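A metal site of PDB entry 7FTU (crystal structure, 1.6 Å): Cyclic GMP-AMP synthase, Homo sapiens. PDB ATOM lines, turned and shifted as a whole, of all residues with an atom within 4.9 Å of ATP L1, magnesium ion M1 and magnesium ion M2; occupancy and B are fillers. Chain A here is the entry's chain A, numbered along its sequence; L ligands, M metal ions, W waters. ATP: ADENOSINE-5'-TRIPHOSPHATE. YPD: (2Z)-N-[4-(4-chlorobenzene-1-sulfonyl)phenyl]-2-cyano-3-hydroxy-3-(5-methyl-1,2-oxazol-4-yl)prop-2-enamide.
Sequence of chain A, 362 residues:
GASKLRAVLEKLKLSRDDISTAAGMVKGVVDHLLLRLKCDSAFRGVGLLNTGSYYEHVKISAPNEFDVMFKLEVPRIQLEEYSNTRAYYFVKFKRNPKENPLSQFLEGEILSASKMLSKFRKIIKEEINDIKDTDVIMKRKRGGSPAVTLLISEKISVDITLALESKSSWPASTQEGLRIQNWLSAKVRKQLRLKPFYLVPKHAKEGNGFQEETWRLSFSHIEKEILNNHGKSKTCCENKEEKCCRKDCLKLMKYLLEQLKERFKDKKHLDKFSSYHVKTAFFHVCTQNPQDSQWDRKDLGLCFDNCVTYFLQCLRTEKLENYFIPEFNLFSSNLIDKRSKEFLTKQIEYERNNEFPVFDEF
The backbone NH (N) of Asp 159 is in hydrogen-bond range of the backbone carbonyl oxygen (O) of Phe 66 (2.8 Å). The side-chain amino group (NZ) of Lys 279 lies within salt-bridge range of the side-chain carboxylate (OE1) of Glu 223 (2.7 Å). The side-chain carboxylate (OE2) of Glu 223 is in hydrogen-bond range of the side-chain hydroxyl (OH) of Tyr 276. N of Lys 59 lies within hydrogen-bond range of O of Ser 53 (3.1 Å). The side-chain amino group (NZ) of Lys 279 lies within salt-bridge range of the side-chain carboxylate (OE2) of Glu 56, 2.6 Å away.
OD2 of Asp 67 binds magnesium ion M2 (2.0 Å). An oxygen (O1G) of ATP L1 is bound to magnesium ion M2. O2B of ATP L1 binds magnesium ion M2 (2.0 Å). The side-chain carboxylate (OE1) of Glu 65 is bound to magnesium ion M2 (2.0 Å). O2A of ATP L1 is bound to magnesium ion M2 (2.0 Å). Water W6 is bound to magnesium ion M2, at 2.2 Å.
Merely in contact with ATP L1: Gly 52 (3.5 Å), Lys 59 (3.9 Å) and Tyr 276 (3.4 Å). The nearest printed residue that does not touch ATP L1 is Asp 159 (4.1 Å).
Of the 18 residues printed, 3 come within 4 Å of magnesium ion M1.
Water W13 lies within hydrogen-bond range of an oxygen (O7) of YPD L2 (2.8 Å) and an oxygen (O5') of ATP L1 (3.1 Å). Water W6 lies within hydrogen-bond range of the side-chain hydroxyl (OG) of Ser 53 (2.7 Å) and the backbone carbonyl oxygen (O) of Glu 65 (2.8 Å). Water W5 bridges an oxygen (O3G) of ATP L1 (2.7 Å) and the side-chain amino group (NZ) of Lys 59 (3.1 Å). Water W14 lies within hydrogen-bond range of N1 of ATP L1 and ND2 of Asn 322. Water W3 lies within hydrogen-bond range of an oxygen (O1A) of ATP L1, the side-chain hydroxyl of Ser 275 and the backbone NH of Tyr 276. Water W1 lies within hydrogen-bond range of OE2 of Glu 223 (2.8 Å), N3 of ATP L1 (3.2 Å) and OH of Tyr 276 (3.5 Å).
Magnesium ion M1 is bound by water W2. OD1 of Asp 67 binds magnesium ion M1, 2.0 Å away. Magnesium ion M1 is bound by OE2 of Glu 65. OD2 of Asp 159 is bound to magnesium ion M1 (2.0 Å). Magnesium ion M1 is bound by water W13, at 2.0 Å. O2A of ATP L1 is bound to magnesium ion M1, at 2.1 Å.
An oxygen (O2') of ATP L1 sits at hydrogen-bond distance from the side-chain hydroxyl of Ser 220, at 2.5 Å. An oxygen (O2') of ATP L1 is in hydrogen-bond range of the side-chain carboxylate (OE1) of Glu 223 (2.6 Å). The backbone NH (N) of Ser 53 sits close to an oxygen (O2B) of ATP L1. The side-chain hydroxyl (OG) of Ser 53 sits at hydrogen-bond distance from an oxygen (O3G) of ATP L1, 2.7 Å away. The side-chain hydroxyl of Ser 275 lies within hydrogen-bond range of an oxygen (O2G) of ATP L1. O3' of ATP L1 is in hydrogen-bond range of NZ of Lys 279 (2.9 Å). NZ of Lys 254 is in salt-bridge range of O3G of ATP L1 (2.9 Å). NH1 of Arg 216 lies close to N3 of ATP L1 (3.5 Å). The guanidinium group (NH2) of Arg 216 lies within hydrogen-bond range of an oxygen (O2) of YPD L2, 2.8 Å away.
An oxygen (O4') of ATP L1 sits close to an oxygen (O7) of YPD L2.
Of the 18 residues printed, 2 come within 4 Å of magnesium ion M2. The nearest printed residue that does not touch magnesium ion M2 is Ser 53 (4.02 Å).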
ATOM      1  N   GLY A  52      -8.783  -3.407  19.351  1.00  0.00           N
ATOM      2  CA  GLY A  52      -8.976  -4.833  19.192  1.00  0.00           C
ATOM      3  C   GLY A  52      -7.721  -5.663  19.470  1.00  0.00           C
ATOM      4  O   GLY A  52      -6.700  -5.141  19.943  1.00  0.00           O
ATOM      5  N   SER A  53      -7.787  -6.949  19.135  1.00  0.00           N
ATOM      6  CA  SER A  53      -6.935  -7.949  19.767  1.00  0.00           C
ATOM      7  C   SER A  53      -5.496  -7.822  19.295  1.00  0.00           C
ATOM      8  O   SER A  53      -4.569  -8.136  20.052  1.00  0.00           O
ATOM      9  CB  SER A  53      -7.467  -9.339  19.541  1.00  0.00           C
ATOM     10  OG  SER A  53      -7.438  -9.692  18.177  1.00  0.00           O
ATOM     11  N   GLU A  56      -3.927  -5.130  21.367  1.00  0.00           N
ATOM     12  CA  GLU A  56      -4.002  -5.525  22.757  1.00  0.00           C
ATOM     13  C   GLU A  56      -3.099  -6.732  23.028  1.00  0.00           C
ATOM     14  O   GLU A  56      -2.992  -7.194  24.158  1.00  0.00           O
ATOM     15  CB  GLU A  56      -5.449  -5.909  23.093  1.00  0.00           C
ATOM     16  CG  GLU A  56      -6.434  -4.748  23.062  1.00  0.00           C
ATOM     17  CD  GLU A  56      -7.896  -5.157  23.017  1.00  0.00           C
ATOM     18  OE1 GLU A  56      -8.181  -6.281  22.565  1.00  0.00           O
ATOM     19  OE2 GLU A  56      -8.756  -4.355  23.467  1.00  0.00           O
ATOM     20  N   LYS A  59      -4.436 -11.249  20.108  1.00  0.00           N
ATOM     21  CA  LYS A  59      -4.744 -11.948  18.876  1.00  0.00           C
ATOM     22  C   LYS A  59      -4.077 -13.322  18.920  1.00  0.00           C
ATOM     23  O   LYS A  59      -2.916 -13.417  19.325  1.00  0.00           O
ATOM     24  CB  LYS A  59      -4.195 -11.154  17.682  1.00  0.00           C
ATOM     25  CG  LYS A  59      -4.549 -11.722  16.319  1.00  0.00           C
ATOM     26  CD  LYS A  59      -5.981 -11.452  15.938  1.00  0.00           C
ATOM     27  CE  LYS A  59      -6.411 -12.155  14.662  1.00  0.00           C
ATOM     28  NZ  LYS A  59      -6.351 -13.626  14.807  1.00  0.00           N
ATOM     29  N   GLU A  65      -6.512 -10.343  11.360  1.00  0.00           N
ATOM     30  CA  GLU A  65      -7.728  -9.558  11.579  1.00  0.00           C
ATOM     31  C   GLU A  65      -7.374  -8.372  12.483  1.00  0.00           C
ATOM     32  O   GLU A  65      -6.942  -8.529  13.627  1.00  0.00           O
ATOM     33  CB  GLU A  65      -8.888 -10.418  12.100  1.00  0.00           C
ATOM     34  CG  GLU A  65     -10.273  -9.753  12.002  1.00  0.00           C
ATOM     35  CD  GLU A  65     -10.773  -8.876  13.153  1.00  0.00           C
ATOM     36  OE1 GLU A  65     -10.063  -8.764  14.159  1.00  0.00           O
ATOM     37  OE2 GLU A  65     -11.893  -8.315  13.053  1.00  0.00           O
ATOM     38  N   PHE A  66      -7.508  -7.177  11.876  1.00  0.00           N
ATOM     39  CA  PHE A  66      -7.211  -5.905  12.509  1.00  0.00           C
ATOM     40  C   PHE A  66      -8.504  -5.110  12.624  1.00  0.00           C
ATOM     41  O   PHE A  66      -9.392  -5.220  11.771  1.00  0.00           O
ATOM     42  CB  PHE A  66      -6.235  -5.065  11.681  1.00  0.00           C
ATOM     43  CG  PHE A  66      -4.843  -5.633  11.562  1.00  0.00           C
ATOM     44  CD1 PHE A  66      -4.612  -6.802  10.846  1.00  0.00           C
ATOM     45  CD2 PHE A  66      -3.768  -5.002  12.158  1.00  0.00           C
ATOM     46  CE1 PHE A  66      -3.337  -7.316  10.733  1.00  0.00           C
ATOM     47  CE2 PHE A  66      -2.491  -5.524  12.051  1.00  0.00           C
ATOM     48  CZ  PHE A  66      -2.276  -6.676  11.328  1.00  0.00           C
ATOM     49  N   ASP A  67      -8.556  -4.289  13.676  1.00  0.00           N
ATOM     50  CA  ASP A  67      -9.684  -3.427  13.923  1.00  0.00           C
ATOM     51  C   ASP A  67      -9.148  -2.009  14.103  1.00  0.00           C
ATOM     52  O   ASP A  67      -8.161  -1.811  14.822  1.00  0.00           O
ATOM     53  CB  ASP A  67     -10.474  -3.898  15.146  1.00  0.00           C
ATOM     54  CG  ASP A  67     -10.913  -5.338  15.034  1.00  0.00           C
ATOM     55  OD1 ASP A  67     -11.963  -5.589  14.383  1.00  0.00           O
ATOM     56  OD2 ASP A  67     -10.197  -6.218  15.614  1.00  0.00           O
ATOM     57  N   ASP A 159     -11.370  -4.603   9.848  1.00  0.00           N
ATOM     58  CA  ASP A 159     -12.631  -3.960  10.183  1.00  0.00           C
ATOM     59  C   ASP A 159     -12.344  -2.499  10.445  1.00  0.00           C
ATOM     60  O   ASP A 159     -11.542  -2.165  11.317  1.00  0.00           O
ATOM     61  CB  ASP A 159     -13.289  -4.586  11.418  1.00  0.00           C
ATOM     62  CG  ASP A 159     -13.779  -6.017  11.240  1.00  0.00           C
ATOM     63  OD1 ASP A 159     -14.033  -6.411  10.060  1.00  0.00           O
ATOM     64  OD2 ASP A 159     -13.872  -6.722  12.281  1.00  0.00           O
ATOM     65  N   ARG A 216     -24.254   3.320  18.728  1.00  0.00           N
ATOM     66  CA  ARG A 216     -23.946   2.606  19.957  1.00  0.00           C
ATOM     67  C   ARG A 216     -22.623   3.088  20.552  1.00  0.00           C
ATOM     68  O   ARG A 216     -21.677   3.377  19.817  1.00  0.00           O
ATOM     69  CB  ARG A 216     -23.854   1.098  19.722  1.00  0.00           C
ATOM     70  CG  ARG A 216     -24.135   0.287  20.981  1.00  0.00           C
ATOM     71  CD  ARG A 216     -23.452  -1.064  21.000  1.00  0.00           C
ATOM     72  NE  ARG A 216     -22.021  -0.854  21.014  1.00  0.00           N
ATOM     73  CZ  ARG A 216     -21.164  -1.384  20.146  1.00  0.00           C
ATOM     74  NH1 ARG A 216     -19.921  -0.937  20.103  1.00  0.00           N
ATOM     75  NH2 ARG A 216     -21.556  -2.308  19.289  1.00  0.00           N
ATOM     76  N   LEU A 217     -22.552   3.156  21.883  1.00  0.00           N
ATOM     77  CA  LEU A 217     -21.319   3.544  22.553  1.00  0.00           C
ATOM     78  C   LEU A 217     -20.231   2.508  22.291  1.00  0.00           C
ATOM     79  O   LEU A 217     -20.514   1.309  22.188  1.00  0.00           O
ATOM     80  CB  LEU A 217     -21.554   3.661  24.071  1.00  0.00           C
ATOM     81  CG  LEU A 217     -22.420   4.825  24.518  1.00  0.00           C
ATOM     82  CD1 LEU A 217     -22.778   4.679  25.991  1.00  0.00           C
ATOM     83  CD2 LEU A 217     -21.716   6.139  24.290  1.00  0.00           C
ATOM     84  N   SER A 220     -13.601   0.910  22.993  1.00  0.00           N
ATOM     85  CA  SER A 220     -12.507   0.063  22.524  1.00  0.00           C
ATOM     86  C   SER A 220     -11.147   0.613  22.936  1.00  0.00           C
ATOM     87  O   SER A 220     -10.195  -0.158  23.130  1.00  0.00           O
ATOM     88  CB  SER A 220     -12.565  -0.107  21.025  1.00  0.00           C
ATOM     89  OG  SER A 220     -13.745  -0.803  20.637  1.00  0.00           O
ATOM     90  N   GLU A 223     -10.611  -0.337  26.605  1.00  0.00           N
ATOM     91  CA  GLU A 223     -10.332  -1.769  26.661  1.00  0.00           C
ATOM     92  C   GLU A 223      -8.870  -2.034  26.338  1.00  0.00           C
ATOM     93  O   GLU A 223      -8.200  -2.839  26.988  1.00  0.00           O
ATOM     94  CB  GLU A 223     -11.254  -2.537  25.703  1.00  0.00           C
ATOM     95  CG  GLU A 223     -12.714  -2.405  26.075  1.00  0.00           C
ATOM     96  CD  GLU A 223     -13.698  -2.996  25.091  1.00  0.00           C
ATOM     97  OE1 GLU A 223     -13.257  -3.654  24.132  1.00  0.00           O
ATOM     98  OE2 GLU A 223     -14.917  -2.772  25.289  1.00  0.00           O
ATOM     99  N   LYS A 254     -10.645 -17.346  24.240  1.00  0.00           N
ATOM    100  CA  LYS A 254     -10.940 -17.023  22.853  1.00  0.00           C
ATOM    101  C   LYS A 254     -10.832 -18.279  21.984  1.00  0.00           C
ATOM    102  O   LYS A 254     -11.708 -18.516  21.153  1.00  0.00           O
ATOM    103  CB  LYS A 254      -9.988 -15.945  22.322  1.00  0.00           C
ATOM    104  CG  LYS A 254     -10.241 -14.557  22.876  1.00  0.00           C
ATOM    105  CD  LYS A 254      -9.118 -13.562  22.646  1.00  0.00           C
ATOM    106  CE  LYS A 254      -8.877 -13.219  21.188  1.00  0.00           C
ATOM    107  NZ  LYS A 254     -10.143 -12.831  20.532  1.00  0.00           N
ATOM    108  N   SER A 275     -16.141 -13.313  20.149  1.00  0.00           N
ATOM    109  CA  SER A 275     -15.001 -13.107  21.014  1.00  0.00           C
ATOM    110  C   SER A 275     -15.260 -12.006  22.035  1.00  0.00           C
ATOM    111  O   SER A 275     -14.719 -12.072  23.138  1.00  0.00           O
ATOM    112  CB  SER A 275     -13.745 -12.853  20.203  1.00  0.00           C
ATOM    113  OG  SER A 275     -13.790 -11.598  19.557  1.00  0.00           O
ATOM    114  N   TYR A 276     -16.084 -10.992  21.705  1.00  0.00           N
ATOM    115  CA  TYR A 276     -16.341  -9.906  22.646  1.00  0.00           C
ATOM    116  C   TYR A 276     -17.066 -10.415  23.898  1.00  0.00           C
ATOM    117  O   TYR A 276     -16.964  -9.811  24.977  1.00  0.00           O
ATOM    118  CB  TYR A 276     -17.138  -8.763  22.005  1.00  0.00           C
ATOM    119  CG  TYR A 276     -17.189  -7.505  22.842  1.00  0.00           C
ATOM    120  CD1 TYR A 276     -16.035  -6.804  23.151  1.00  0.00           C
ATOM    121  CD2 TYR A 276     -18.372  -7.049  23.404  1.00  0.00           C
ATOM    122  CE1 TYR A 276     -16.056  -5.677  23.955  1.00  0.00           C
ATOM    123  CE2 TYR A 276     -18.413  -5.930  24.219  1.00  0.00           C
ATOM    124  CZ  TYR A 276     -17.244  -5.228  24.494  1.00  0.00           C
ATOM    125  OH  TYR A 276     -17.232  -4.101  25.285  1.00  0.00           O
ATOM    126  N   LYS A 279     -14.210 -11.706  25.978  1.00  0.00           N
ATOM    127  CA  LYS A 279     -13.470 -10.539  26.442  1.00  0.00           C
ATOM    128  C   LYS A 279     -14.186  -9.868  27.613  1.00  0.00           C
ATOM    129  O   LYS A 279     -13.547  -9.530  28.604  1.00  0.00           O
ATOM    130  CB  LYS A 279     -13.277  -9.530  25.313  1.00  0.00           C
ATOM    131  CG  LYS A 279     -12.220  -8.466  25.571  1.00  0.00           C
ATOM    132  CD  LYS A 279     -12.252  -7.360  24.518  1.00  0.00           C
ATOM    133  CE  LYS A 279     -11.091  -6.386  24.608  1.00  0.00           C
ATOM    134  NZ  LYS A 279     -11.189  -5.316  23.597  1.00  0.00           N
ATOM    135  N   ASN A 322     -22.338  -5.588  29.764  1.00  0.00           N
ATOM    136  CA  ASN A 322     -21.313  -4.771  29.158  1.00  0.00           C
ATOM    137  C   ASN A 322     -20.461  -4.183  30.291  1.00  0.00           C
ATOM    138  O   ASN A 322     -20.974  -3.724  31.308  1.00  0.00           O
ATOM    139  CB  ASN A 322     -21.969  -3.733  28.257  1.00  0.00           C
ATOM    140  CG  ASN A 322     -20.960  -2.826  27.589  1.00  0.00           C
ATOM    141  OD1 ASN A 322     -20.325  -2.013  28.256  1.00  0.00           O
ATOM    142  ND2 ASN A 322     -20.834  -2.913  26.283  1.00  0.00           N
ATOM    143  N   LEU A 330     -25.542  -8.316  27.257  1.00  0.00           N
ATOM    144  CA  LEU A 330     -25.159  -8.900  25.982  1.00  0.00           C
ATOM    145  C   LEU A 330     -25.831 -10.261  25.772  1.00  0.00           C
ATOM    146  O   LEU A 330     -25.884 -10.750  24.636  1.00  0.00           O
ATOM    147  CB  LEU A 330     -23.633  -9.065  25.924  1.00  0.00           C
ATOM    148  CG  LEU A 330     -22.785  -7.795  26.114  1.00  0.00           C
ATOM    149  CD1 LEU A 330     -21.308  -8.124  26.070  1.00  0.00           C
ATOM    150  CD2 LEU A 330     -23.105  -6.753  25.064  1.00  0.00           C
HETATM  151  PG  ATP L   1     -10.613 -11.009  17.749  1.00  0.00           P
HETATM  152  O1G ATP L   1     -10.649 -10.059  16.564  1.00  0.00           O
HETATM  153  O2G ATP L   1     -11.740 -11.975  17.812  1.00  0.00           O
HETATM  154  O3G ATP L   1      -9.278 -11.646  18.004  1.00  0.00           O
HETATM  155  PB  ATP L   1     -11.275  -8.487  19.005  1.00  0.00           P
HETATM  156  O1B ATP L   1     -11.343  -7.955  20.415  1.00  0.00           O
HETATM  157  O2B ATP L   1     -10.426  -7.747  17.994  1.00  0.00           O
HETATM  158  O3B ATP L   1     -10.868 -10.018  19.014  1.00  0.00           O
HETATM  159  PA  ATP L   1     -13.456  -7.943  17.125  1.00  0.00           P
HETATM  160  O1A ATP L   1     -14.674  -8.782  16.896  1.00  0.00           O
HETATM  161  O2A ATP L   1     -12.479  -7.765  15.973  1.00  0.00           O
HETATM  162  O3A ATP L   1     -12.743  -8.605  18.393  1.00  0.00           O
HETATM  163  O5' ATP L   1     -13.883  -6.526  17.707  1.00  0.00           O
HETATM  164  C5' ATP L   1     -12.915  -5.466  17.802  1.00  0.00           C
HETATM  165  C4' ATP L   1     -13.288  -4.588  18.962  1.00  0.00           C
HETATM  166  O4' ATP L   1     -14.619  -4.058  18.738  1.00  0.00           O
HETATM  167  C3' ATP L   1     -13.406  -5.263  20.326  1.00  0.00           C
HETATM  168  O3' ATP L   1     -12.124  -5.471  20.903  1.00  0.00           O
HETATM  169  C2' ATP L   1     -14.279  -4.249  21.069  1.00  0.00           C
HETATM  170  O2' ATP L   1     -13.549  -3.149  21.554  1.00  0.00           O
HETATM  171  C1' ATP L   1     -15.250  -3.808  19.974  1.00  0.00           C
HETATM  172  N9  ATP L   1     -16.511  -4.539  19.976  1.00  0.00           N
HETATM  173  C8  ATP L   1     -16.807  -5.675  19.266  1.00  0.00           C
HETATM  174  N7  ATP L   1     -18.027  -6.091  19.491  1.00  0.00           N
HETATM  175  C5  ATP L   1     -18.545  -5.185  20.402  1.00  0.00           C
HETATM  176  C6  ATP L   1     -19.805  -5.092  21.039  1.00  0.00           C
HETATM  177  N6  ATP L   1     -20.789  -5.966  20.850  1.00  0.00           N
HETATM  178  N1  ATP L   1     -19.998  -4.064  21.892  1.00  0.00           N
HETATM  179  C2  ATP L   1     -18.986  -3.212  22.109  1.00  0.00           C
HETATM  180  N3  ATP L   1     -17.766  -3.201  21.574  1.00  0.00           N
HETATM  181  C4  ATP L   1     -17.615  -4.229  20.718  1.00  0.00           C
HETATM  182  C13 YPD L   2     -13.699  -2.181  13.953  1.00  0.00           C
HETATM  183  C15 YPD L   2     -19.433  -4.949  16.073  1.00  0.00           C
HETATM  184  C16 YPD L   2     -19.419  -5.658  14.882  1.00  0.00           C
HETATM  185  C17 YPD L   2     -20.484  -6.473  14.537  1.00  0.00           C
HETATM  186  C18 YPD L   2     -21.561  -6.589  15.404  1.00  0.00           C
HETATM  187  C19 YPD L   2     -21.589  -5.902  16.607  1.00  0.00           C
HETATM  188  C20 YPD L   2     -20.514  -5.081  16.938  1.00  0.00           C
HETATM  189  C22 YPD L   2     -22.465  -9.264  15.409  1.00  0.00           C
HETATM  190  C23 YPD L   2     -23.053  -9.867  16.509  1.00  0.00           C
HETATM  191  C24 YPD L   2     -22.686 -11.156  16.857  1.00  0.00           C
HETATM  192  C25 YPD L   2     -21.747 -11.824  16.099  1.00  0.00           C
HETATM  193  C26 YPD L   2     -21.156 -11.228  15.006  1.00  0.00           C
HETATM  194  C27 YPD L   2     -21.514  -9.937  14.658  1.00  0.00           C
HETATM  195  C1  YPD L   2     -18.199  -3.085  17.224  1.00  0.00           C
HETATM  196  O2  YPD L   2     -19.083  -2.780  18.030  1.00  0.00           O
HETATM  197  C3  YPD L   2     -16.949  -2.319  17.205  1.00  0.00           C
HETATM  198  C4  YPD L   2     -16.862  -1.218  18.097  1.00  0.00           C
HETATM  199  N5  YPD L   2     -16.834  -0.346  18.825  1.00  0.00           N
HETATM  200  C6  YPD L   2     -15.853  -2.589  16.402  1.00  0.00           C
HETATM  201  O7  YPD L   2     -15.868  -3.605  15.552  1.00  0.00           O
HETATM  202  C8  YPD L   2     -14.582  -1.854  16.401  1.00  0.00           C
HETATM  203  C9  YPD L   2     -13.709  -1.717  15.359  1.00  0.00           C
HETATM  204  O10 YPD L   2     -12.664  -0.975  15.752  1.00  0.00           O
HETATM  205  N11 YPD L   2     -12.825  -0.610  17.109  1.00  0.00           N
HETATM  206  C12 YPD L   2     -13.955  -1.155  17.454  1.00  0.00           C
HETATM  207  N14 YPD L   2     -18.304  -4.142  16.357  1.00  0.00           N
HETATM  208  S21 YPD L   2     -22.920  -7.621  14.952  1.00  0.00           S
HETATM  209 CL28 YPD L   2     -21.287 -13.440  16.523  1.00  0.00          CL
HETATM  210  O29 YPD L   2     -24.057  -7.245  15.765  1.00  0.00           O
HETATM  211  O30 YPD L   2     -23.046  -7.572  13.524  1.00  0.00           O
HETATM  212 MG    MG M   1     -13.163  -7.163  14.130  1.00  0.00          MG
HETATM  213 MG    MG M   2     -10.469  -8.143  16.029  1.00  0.00          MG
HETATM  214  O   HOH W   1     -16.522  -1.114  23.678  1.00  0.00           O
HETATM  215  O   HOH W   2     -14.373  -8.723  14.020  1.00  0.00           O
HETATM  216  O   HOH W   3     -16.398 -10.046  18.691  1.00  0.00           O
HETATM  217  O   HOH W   4     -13.245  -9.686  21.483  1.00  0.00           O
HETATM  218  O   HOH W   5      -7.704 -13.754  17.630  1.00  0.00           O
HETATM  219  O   HOH W   6      -8.281  -8.257  16.018  1.00  0.00           O
HETATM  220  O   HOH W   7     -18.577  -8.406  18.225  1.00  0.00           O
HETATM  221  O   HOH W   8     -20.727  -8.950  19.490  1.00  0.00           O
HETATM  222  O   HOH W   9      -9.528  -8.649  22.334  1.00  0.00           O
HETATM  223  O   HOH W  10     -11.725 -11.419  14.275  1.00  0.00           O
HETATM  224  O   HOH W  11     -11.193 -14.891  19.142  1.00  0.00           O
HETATM  225  O   HOH W  12     -17.076  -7.829  15.868  1.00  0.00           O
HETATM  226  O   HOH W  13     -14.718  -6.022  14.788  1.00  0.00           O
HETATM  227  O   HOH W  14     -21.989  -3.768  23.774  1.00  0.00           O
